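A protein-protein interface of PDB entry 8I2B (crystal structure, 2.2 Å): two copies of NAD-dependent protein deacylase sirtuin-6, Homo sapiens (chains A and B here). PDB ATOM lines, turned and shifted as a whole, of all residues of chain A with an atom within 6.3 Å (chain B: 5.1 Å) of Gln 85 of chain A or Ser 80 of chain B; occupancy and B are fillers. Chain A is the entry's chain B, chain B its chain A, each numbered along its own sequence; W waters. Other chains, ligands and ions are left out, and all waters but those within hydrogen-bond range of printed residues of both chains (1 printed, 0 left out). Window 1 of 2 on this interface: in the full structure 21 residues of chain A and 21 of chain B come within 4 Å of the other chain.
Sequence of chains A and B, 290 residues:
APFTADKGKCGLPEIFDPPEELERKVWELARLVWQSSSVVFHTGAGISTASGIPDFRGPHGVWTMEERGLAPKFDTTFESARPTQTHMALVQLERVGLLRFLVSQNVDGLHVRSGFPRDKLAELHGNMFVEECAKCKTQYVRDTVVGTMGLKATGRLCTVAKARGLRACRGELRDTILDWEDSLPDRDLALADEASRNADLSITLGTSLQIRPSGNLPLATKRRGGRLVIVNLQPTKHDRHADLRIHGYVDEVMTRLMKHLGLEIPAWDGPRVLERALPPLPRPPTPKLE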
ATOM      1  N   ARG A  82      25.186 -24.610 -10.294  1.00  0.00           N
ATOM      2  CA  ARG A  82      24.209 -25.399  -9.513  1.00  0.00           C
ATOM      3  C   ARG A  82      23.272 -24.419  -8.812  1.00  0.00           C
ATOM      4  O   ARG A  82      23.683 -23.382  -8.291  1.00  0.00           O
ATOM      5  CB  ARG A  82      24.893 -26.419  -8.590  1.00  0.00           C
ATOM      6  CG  ARG A  82      25.469 -25.891  -7.286  1.00  0.00           C
ATOM      7  CD  ARG A  82      25.567 -27.060  -6.296  1.00  0.00           C
ATOM      8  NE  ARG A  82      24.233 -27.356  -5.769  1.00  0.00           N
ATOM      9  CZ  ARG A  82      23.737 -28.547  -5.435  1.00  0.00           C
ATOM     10  NH1 ARG A  82      24.443 -29.658  -5.595  1.00  0.00           N
ATOM     11  NH2 ARG A  82      22.503 -28.622  -4.936  1.00  0.00           N
ATOM     12  N   PRO A  83      21.981 -24.769  -8.763  1.00  0.00           N
ATOM     13  CA  PRO A  83      21.031 -24.052  -7.926  1.00  0.00           C
ATOM     14  C   PRO A  83      21.532 -23.970  -6.484  1.00  0.00           C
ATOM     15  O   PRO A  83      22.114 -24.949  -5.984  1.00  0.00           O
ATOM     16  CB  PRO A  83      19.774 -24.919  -7.979  1.00  0.00           C
ATOM     17  CG  PRO A  83      19.915 -25.702  -9.284  1.00  0.00           C
ATOM     18  CD  PRO A  83      21.397 -25.953  -9.434  1.00  0.00           C
ATOM     19  N   THR A  84      21.296 -22.816  -5.866  1.00  0.00           N
ATOM     20  CA  THR A  84      21.657 -22.532  -4.473  1.00  0.00           C
ATOM     21  C   THR A  84      20.666 -23.254  -3.567  1.00  0.00           C
ATOM     22  O   THR A  84      19.536 -23.648  -4.047  1.00  0.00           O
ATOM     23  CB  THR A  84      21.592 -21.033  -4.168  1.00  0.00           C
ATOM     24  OG1 THR A  84      20.231 -20.583  -4.309  1.00  0.00           O
ATOM     25  CG2 THR A  84      22.494 -20.234  -5.074  1.00  0.00           C
ATOM     26  N   GLN A  85      21.038 -23.345  -2.309  1.00  0.00           N
ATOM     27  CA  GLN A  85      20.114 -23.673  -1.189  1.00  0.00           C
ATOM     28  C   GLN A  85      18.772 -22.887  -1.347  1.00  0.00           C
ATOM     29  O   GLN A  85      17.736 -23.470  -1.123  1.00  0.00           O
ATOM     30  CB  GLN A  85      20.895 -23.351   0.081  1.00  0.00           C
ATOM     31  CG  GLN A  85      22.099 -24.291   0.276  1.00  0.00           C
ATOM     32  CD  GLN A  85      22.932 -23.959   1.497  1.00  0.00           C
ATOM     33  OE1 GLN A  85      22.960 -24.701   2.480  1.00  0.00           O
ATOM     34  NE2 GLN A  85      23.635 -22.832   1.464  1.00  0.00           N
ATOM     35  N   THR A  86      18.795 -21.588  -1.682  1.00  0.00           N
ATOM     36  CA  THR A  86      17.564 -20.767  -1.842  1.00  0.00           C
ATOM     37  C   THR A  86      16.713 -21.348  -2.970  1.00  0.00           C
ATOM     38  O   THR A  86      15.549 -21.585  -2.738  1.00  0.00           O
ATOM     39  CB  THR A  86      17.862 -19.285  -2.093  1.00  0.00           C
ATOM     40  OG1 THR A  86      18.391 -18.812  -0.862  1.00  0.00           O
ATOM     41  CG2 THR A  86      16.624 -18.498  -2.469  1.00  0.00           C
ATOM     42  N   HIS A  87      17.308 -21.652  -4.120  1.00  0.00           N
ATOM     43  CA  HIS A  87      16.611 -22.272  -5.270  1.00  0.00           C
ATOM     44  C   HIS A  87      15.890 -23.542  -4.812  1.00  0.00           C
ATOM     45  O   HIS A  87      14.728 -23.796  -5.191  1.00  0.00           O
ATOM     46  CB  HIS A  87      17.571 -22.612  -6.409  1.00  0.00           C
ATOM     47  CG  HIS A  87      17.993 -21.448  -7.244  1.00  0.00           C
ATOM     48  ND1 HIS A  87      19.183 -20.784  -7.018  1.00  0.00           N
ATOM     49  CD2 HIS A  87      17.405 -20.831  -8.301  1.00  0.00           C
ATOM     50  CE1 HIS A  87      19.337 -19.822  -7.927  1.00  0.00           C
ATOM     51  NE2 HIS A  87      18.262 -19.809  -8.703  1.00  0.00           N
ATOM     52  N   MET A  88      16.603 -24.386  -4.096  1.00  0.00           N
ATOM     53  CA  MET A  88      16.095 -25.706  -3.691  1.00  0.00           C
ATOM     54  C   MET A  88      15.067 -25.519  -2.585  1.00  0.00           C
ATOM     55  O   MET A  88      14.132 -26.298  -2.532  1.00  0.00           O
ATOM     56  CB  MET A  88      17.261 -26.597  -3.213  1.00  0.00           C
ATOM     57  CG  MET A  88      18.228 -26.963  -4.331  1.00  0.00           C
ATOM     58  SD  MET A  88      17.427 -27.375  -5.969  1.00  0.00           S
ATOM     59  CE  MET A  88      16.515 -28.860  -5.578  1.00  0.00           C
ATOM     60  N   ALA A  89      15.211 -24.503  -1.729  1.00  0.00           N
ATOM     61  CA  ALA A  89      14.194 -24.234  -0.697  1.00  0.00           C
ATOM     62  C   ALA A  89      12.886 -23.807  -1.396  1.00  0.00           C
ATOM     63  O   ALA A  89      11.835 -24.159  -0.903  1.00  0.00           O
ATOM     64  CB  ALA A  89      14.698 -23.173   0.236  1.00  0.00           C
ATOM     65  N   LEU A  90      12.961 -23.102  -2.536  1.00  0.00           N
ATOM     66  CA  LEU A  90      11.741 -22.641  -3.252  1.00  0.00           C
ATOM     67  C   LEU A  90      11.053 -23.855  -3.876  1.00  0.00           C
ATOM     68  O   LEU A  90       9.812 -23.887  -3.827  1.00  0.00           O
ATOM     69  CB  LEU A  90      12.112 -21.578  -4.272  1.00  0.00           C
ATOM     70  CG  LEU A  90      12.611 -20.297  -3.606  1.00  0.00           C
ATOM     71  CD1 LEU A  90      13.330 -19.427  -4.589  1.00  0.00           C
ATOM     72  CD2 LEU A  90      11.474 -19.555  -2.909  1.00  0.00           C
ATOM     73  N   TYR A 249      22.391 -12.509   3.686  1.00  0.00           N
ATOM     74  CA  TYR A 249      22.502 -13.565   2.640  1.00  0.00           C
ATOM     75  C   TYR A 249      21.214 -14.395   2.581  1.00  0.00           C
ATOM     76  O   TYR A 249      20.783 -14.868   3.648  1.00  0.00           O
ATOM     77  CB  TYR A 249      23.735 -14.407   2.959  1.00  0.00           C
ATOM     78  CG  TYR A 249      25.010 -13.599   2.931  1.00  0.00           C
ATOM     79  CD1 TYR A 249      25.466 -13.050   1.755  1.00  0.00           C
ATOM     80  CD2 TYR A 249      25.714 -13.316   4.089  1.00  0.00           C
ATOM     81  CE1 TYR A 249      26.630 -12.313   1.691  1.00  0.00           C
ATOM     82  CE2 TYR A 249      26.900 -12.605   4.054  1.00  0.00           C
ATOM     83  CZ  TYR A 249      27.371 -12.125   2.839  1.00  0.00           C
ATOM     84  OH  TYR A 249      28.489 -11.368   2.748  1.00  0.00           O
ATOM     85  N   ASP A 251      20.555 -17.275   1.289  1.00  0.00           N
ATOM     86  CA  ASP A 251      20.865 -18.672   1.688  1.00  0.00           C
ATOM     87  C   ASP A 251      20.682 -18.836   3.204  1.00  0.00           C
ATOM     88  O   ASP A 251      20.003 -19.780   3.614  1.00  0.00           O
ATOM     89  CB  ASP A 251      22.246 -19.034   1.131  1.00  0.00           C
ATOM     90  CG  ASP A 251      22.136 -19.523  -0.282  1.00  0.00           C
ATOM     91  OD1 ASP A 251      20.956 -19.555  -0.824  1.00  0.00           O
ATOM     92  OD2 ASP A 251      23.210 -19.804  -0.853  1.00  0.00           O
ATOM     93  N   GLU A 252      21.135 -17.870   4.000  1.00  0.00           N
ATOM     94  CA  GLU A 252      21.079 -17.955   5.487  1.00  0.00           C
ATOM     95  C   GLU A 252      19.627 -17.737   5.946  1.00  0.00           C
ATOM     96  O   GLU A 252      19.072 -18.515   6.711  1.00  0.00           O
ATOM     97  CB  GLU A 252      22.089 -16.949   6.063  1.00  0.00           C
ATOM     98  CG  GLU A 252      22.498 -17.291   7.488  1.00  0.00           C
ATOM     99  CD  GLU A 252      23.691 -16.533   8.058  1.00  0.00           C
ATOM    100  OE1 GLU A 252      24.826 -17.141   8.178  1.00  0.00           O
ATOM    101  OE2 GLU A 252      23.483 -15.360   8.425  1.00  0.00           O
ATOM    102  N   VAL A 253      18.997 -16.692   5.455  1.00  0.00           N
ATOM    103  CA  VAL A 253      17.552 -16.427   5.696  1.00  0.00           C
ATOM    104  C   VAL A 253      16.736 -17.676   5.361  1.00  0.00           C
ATOM    105  O   VAL A 253      15.959 -18.163   6.230  1.00  0.00           O
ATOM    106  CB  VAL A 253      17.107 -15.205   4.873  1.00  0.00           C
ATOM    107  CG1 VAL A 253      15.593 -15.115   4.882  1.00  0.00           C
ATOM    108  CG2 VAL A 253      17.783 -13.939   5.393  1.00  0.00           C
ATOM    109  N   MET A 254      16.893 -18.222   4.166  1.00  0.00           N
ATOM    110  CA  MET A 254      16.021 -19.345   3.721  1.00  0.00           C
ATOM    111  C   MET A 254      16.341 -20.644   4.467  1.00  0.00           C
ATOM    112  O   MET A 254      15.387 -21.380   4.757  1.00  0.00           O
ATOM    113  CB  MET A 254      16.120 -19.548   2.212  1.00  0.00           C
ATOM    114  CG  MET A 254      15.592 -18.328   1.443  1.00  0.00           C
ATOM    115  SD  MET A 254      13.813 -18.170   1.687  1.00  0.00           S
ATOM    116  CE  MET A 254      13.217 -19.523   0.687  1.00  0.00           C
ATOM    117  N   THR A 255      17.595 -20.949   4.807  1.00  0.00           N
ATOM    118  CA  THR A 255      17.917 -22.167   5.608  1.00  0.00           C
ATOM    119  C   THR A 255      17.335 -22.009   7.013  1.00  0.00           C
ATOM    120  O   THR A 255      16.761 -22.967   7.539  1.00  0.00           O
ATOM    121  CB  THR A 255      19.428 -22.475   5.676  1.00  0.00           C
ATOM    122  OG1 THR A 255      20.083 -21.431   6.381  1.00  0.00           O
ATOM    123  CG2 THR A 255      20.090 -22.589   4.326  1.00  0.00           C
ATOM    124  N   ARG A 256      17.425 -20.839   7.642  1.00  0.00           N
ATOM    125  CA  ARG A 256      16.743 -20.670   8.963  1.00  0.00           C
ATOM    126  C   ARG A 256      15.219 -20.764   8.794  1.00  0.00           C
ATOM    127  O   ARG A 256      14.557 -21.384   9.660  1.00  0.00           O
ATOM    128  CB  ARG A 256      17.092 -19.325   9.615  1.00  0.00           C
ATOM    129  CG  ARG A 256      18.517 -19.300  10.145  1.00  0.00           C
ATOM    130  CD  ARG A 256      19.069 -17.908  10.375  1.00  0.00           C
ATOM    131  NE  ARG A 256      20.474 -18.027  10.723  1.00  0.00           N
ATOM    132  CZ  ARG A 256      21.182 -17.143  11.414  1.00  0.00           C
ATOM    133  NH1 ARG A 256      20.621 -16.041  11.894  1.00  0.00           N
ATOM    134  NH2 ARG A 256      22.458 -17.392  11.651  1.00  0.00           N
ATOM    135  N   ILE A 265      15.583 -29.123   2.861  1.00  0.00           N
ATOM    136  CA  ILE A 265      15.947 -28.622   1.520  1.00  0.00           C
ATOM    137  C   ILE A 265      16.341 -29.845   0.708  1.00  0.00           C
ATOM    138  O   ILE A 265      17.298 -30.543   1.032  1.00  0.00           O
ATOM    139  CB  ILE A 265      17.053 -27.564   1.670  1.00  0.00           C
ATOM    140  CG1 ILE A 265      16.471 -26.332   2.372  1.00  0.00           C
ATOM    141  CG2 ILE A 265      17.695 -27.247   0.335  1.00  0.00           C
ATOM    142  CD1 ILE A 265      17.471 -25.248   2.702  1.00  0.00           C
ATOM    143  N   THR B  76      28.385 -15.244   0.573  1.00  0.00           N
ATOM    144  CA  THR B  76      27.967 -16.167   1.648  1.00  0.00           C
ATOM    145  C   THR B  76      28.833 -15.897   2.868  1.00  0.00           C
ATOM    146  O   THR B  76      29.874 -15.231   2.708  1.00  0.00           O
ATOM    147  CB  THR B  76      28.117 -17.644   1.220  1.00  0.00           C
ATOM    148  OG1 THR B  76      27.663 -18.410   2.331  1.00  0.00           O
ATOM    149  CG2 THR B  76      29.536 -18.075   0.907  1.00  0.00           C
ATOM    150  N   THR B  77      28.412 -16.379   4.042  1.00  0.00           N
ATOM    151  CA  THR B  77      29.286 -16.503   5.223  1.00  0.00           C
ATOM    152  C   THR B  77      29.973 -17.861   5.146  1.00  0.00           C
ATOM    153  O   THR B  77      29.517 -18.759   4.349  1.00  0.00           O
ATOM    154  CB  THR B  77      28.542 -16.408   6.558  1.00  0.00           C
ATOM    155  OG1 THR B  77      27.584 -17.457   6.506  1.00  0.00           O
ATOM    156  CG2 THR B  77      27.889 -15.075   6.848  1.00  0.00           C
ATOM    157  N   PHE B  78      30.987 -18.056   5.979  1.00  0.00           N
ATOM    158  CA  PHE B  78      31.683 -19.362   6.076  1.00  0.00           C
ATOM    159  C   PHE B  78      30.688 -20.418   6.532  1.00  0.00           C
ATOM    160  O   PHE B  78      30.720 -21.535   5.979  1.00  0.00           O
ATOM    161  CB  PHE B  78      32.925 -19.270   6.966  1.00  0.00           C
ATOM    162  CG  PHE B  78      34.045 -18.542   6.279  1.00  0.00           C
ATOM    163  CD1 PHE B  78      34.688 -19.131   5.206  1.00  0.00           C
ATOM    164  CD2 PHE B  78      34.403 -17.260   6.638  1.00  0.00           C
ATOM    165  CE1 PHE B  78      35.666 -18.447   4.509  1.00  0.00           C
ATOM    166  CE2 PHE B  78      35.410 -16.593   5.961  1.00  0.00           C
ATOM    167  CZ  PHE B  78      36.037 -17.193   4.901  1.00  0.00           C
ATOM    168  N   GLU B  79      29.802 -20.050   7.461  1.00  0.00           N
ATOM    169  CA  GLU B  79      28.829 -20.985   8.071  1.00  0.00           C
ATOM    170  C   GLU B  79      27.739 -21.388   7.075  1.00  0.00           C
ATOM    171  O   GLU B  79      27.294 -22.509   7.196  1.00  0.00           O
ATOM    172  CB  GLU B  79      28.137 -20.349   9.287  1.00  0.00           C
ATOM    173  CG  GLU B  79      29.076 -20.189  10.458  1.00  0.00           C
ATOM    174  CD  GLU B  79      29.884 -18.906  10.502  1.00  0.00           C
ATOM    175  OE1 GLU B  79      29.756 -18.053   9.551  1.00  0.00           O
ATOM    176  OE2 GLU B  79      30.640 -18.767  11.486  1.00  0.00           O
ATOM    177  N   SER B  80      27.252 -20.484   6.218  1.00  0.00           N
ATOM    178  CA  SER B  80      26.144 -20.779   5.257  1.00  0.00           C
ATOM    179  C   SER B  80      26.698 -21.279   3.908  1.00  0.00           C
ATOM    180  O   SER B  80      25.906 -21.641   3.021  1.00  0.00           O
ATOM    181  CB  SER B  80      25.287 -19.587   5.041  1.00  0.00           C
ATOM    182  OG  SER B  80      24.629 -19.232   6.250  1.00  0.00           O
ATOM    183  N   ALA B  81      28.013 -21.299   3.734  1.00  0.00           N
ATOM    184  CA  ALA B  81      28.606 -21.765   2.449  1.00  0.00           C
ATOM    185  C   ALA B  81      28.316 -23.265   2.299  1.00  0.00           C
ATOM    186  O   ALA B  81      28.391 -24.027   3.302  1.00  0.00           O
ATOM    187  CB  ALA B  81      30.077 -21.502   2.403  1.00  0.00           C
ATOM    188  N   ARG B  82      28.007 -23.694   1.096  1.00  0.00           N
ATOM    189  CA  ARG B  82      27.827 -25.114   0.746  1.00  0.00           C
ATOM    190  C   ARG B  82      29.039 -25.556  -0.066  1.00  0.00           C
ATOM    191  O   ARG B  82      29.538 -24.843  -0.934  1.00  0.00           O
ATOM    192  CB  ARG B  82      26.496 -25.352   0.024  1.00  0.00           C
ATOM    193  CG  ARG B  82      26.395 -24.891  -1.422  1.00  0.00           C
ATOM    194  CD  ARG B  82      25.345 -25.723  -2.152  1.00  0.00           C
ATOM    195  NE  ARG B  82      25.718 -27.138  -2.316  1.00  0.00           N
ATOM    196  CZ  ARG B  82      24.955 -28.206  -2.049  1.00  0.00           C
ATOM    197  NH1 ARG B  82      23.740 -28.075  -1.547  1.00  0.00           N
ATOM    198  NH2 ARG B  82      25.437 -29.427  -2.247  1.00  0.00           N
ATOM    199  N   TRP B 268      24.821 -33.591  -0.449  1.00  0.00           N
ATOM    200  CA  TRP B 268      25.379 -33.060   0.819  1.00  0.00           C
ATOM    201  C   TRP B 268      24.243 -32.956   1.826  1.00  0.00           C
ATOM    202  O   TRP B 268      23.284 -32.217   1.555  1.00  0.00           O
ATOM    203  CB  TRP B 268      26.068 -31.702   0.602  1.00  0.00           C
ATOM    204  CG  TRP B 268      26.693 -31.118   1.829  1.00  0.00           C
ATOM    205  CD1 TRP B 268      27.690 -31.664   2.590  1.00  0.00           C
ATOM    206  CD2 TRP B 268      26.348 -29.866   2.446  1.00  0.00           C
ATOM    207  NE1 TRP B 268      28.032 -30.817   3.603  1.00  0.00           N
ATOM    208  CE2 TRP B 268      27.240 -29.693   3.523  1.00  0.00           C
ATOM    209  CE3 TRP B 268      25.439 -28.836   2.138  1.00  0.00           C
ATOM    210  CZ2 TRP B 268      27.197 -28.553   4.328  1.00  0.00           C
ATOM    211  CZ3 TRP B 268      25.414 -27.691   2.919  1.00  0.00           C
ATOM    212  CH2 TRP B 268      26.263 -27.571   4.020  1.00  0.00           C
HETATM  213  O   HOH W   1      25.450 -20.157   0.618  1.00  0.00           O
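OG1 of Thr 77 of chain B is in hydrogen-bond range of OE1 of Glu 252 of chain A, 3.2 Å away. OE1 of Glu 252 of chain A is in hydrogen-bond range of OG of Ser 80 of chain B (2.9 Å). O of Ser 80 of chain B lies within hydrogen-bond range of NE2 of Gln 85 of chain A, at 3.0 Å.
Water W1 lies within hydrogen-bond range of the side-chain carboxylate of Asp 251 of chain A (2.7 Å), the backbone carbonyl oxygen of Ser 80 of chain B (2.9 Å), the side-chain hydroxyl of Thr 76 of chain B (3.3 Å) and the side-chain amide nitrogen of Gln 85 of chain A (3.3 Å).
The side-chain carboxylate (OE2) of Glu 252 of chain A is in salt-bridge range of the guanidinium group (NH2) of Arg 256 of chain A, 3.9 Å away. The side-chain hydroxyl (OG1) of Thr 77 of chain B sits at hydrogen-bond distance from the backbone NH (N) of Ser 80 of chain B, at 3.1 Å. The side-chain hydroxyl (OG1) of Thr 255 of chain A is in hydrogen-bond range of the backbone carbonyl oxygen (O) of Glu 252 of chain A, at 3.1 Å. The side-chain hydroxyl of Thr 76 of chain B lies within hydrogen-bond range of the backbone NH of Ala 81 of chain B.
Arg 82 of chain A touches its own counterpart, Arg 82 of chain B. Of the 7 pairs that touch across the chains among the printed residues, 1 has its exchanged pair printed and touching as well.
Among the printed residues, pairs that only touch across the chains: Arg 82 of chain A with Arg 82 of chain B (3.5 Å), Gln 85 of chain A with Trp 268 of chain B (3.9 Å), Tyr 249 of chain A with Thr 76 of chain B (3.6 Å) and Tyr 249 of chain A with Thr 77 of chain B (3.9 Å).
Of the 17 printed residues of chain A, 4 touch a printed residue of chain B. Hydrophobic or aromatic side chains of chain A within 4 Å of the printed part of chain B: Tyr 249. Of the 8 printed residues of chain B, 5 touch a printed residue of chain A. Printed residues of chain B that touch a printed residue of chain A: Thr 76, Thr 77, Ser 80, Arg 82 and Trp 268. Among the printed residues, no Asp or Glu carboxylate lies within 4 Å of a Lys or Arg side-chain nitrogen of the other chain.
Of chain B, only Ser 80 and Trp 268 come within 4 Å of Gln 85 of chain A. Ala 89 of chain A touches none of the printed residues of chain B. Of the printed residues of chain B, Tyr 249 of chain A touches Thr 76 (3.6 Å) and Thr 77 (3.9 Å). Of the printed residues of chain B, Glu 252 of chain A touches Thr 77 (3.2 Å) and Ser 80 (2.9 Å). Arg 256 of chain A touches none of the printed residues of chain B. Printed residues of chain A within 4 Å of Thr 77 of chain B: Tyr 249 and Glu 252. Ser 80 of chain B touches just these residues of chain A: Gln 85 and Glu 252. The nearest printed residue of chain A that does not touch Arg 82 of chain B is Gln 85 of chain A (4.1 Å).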
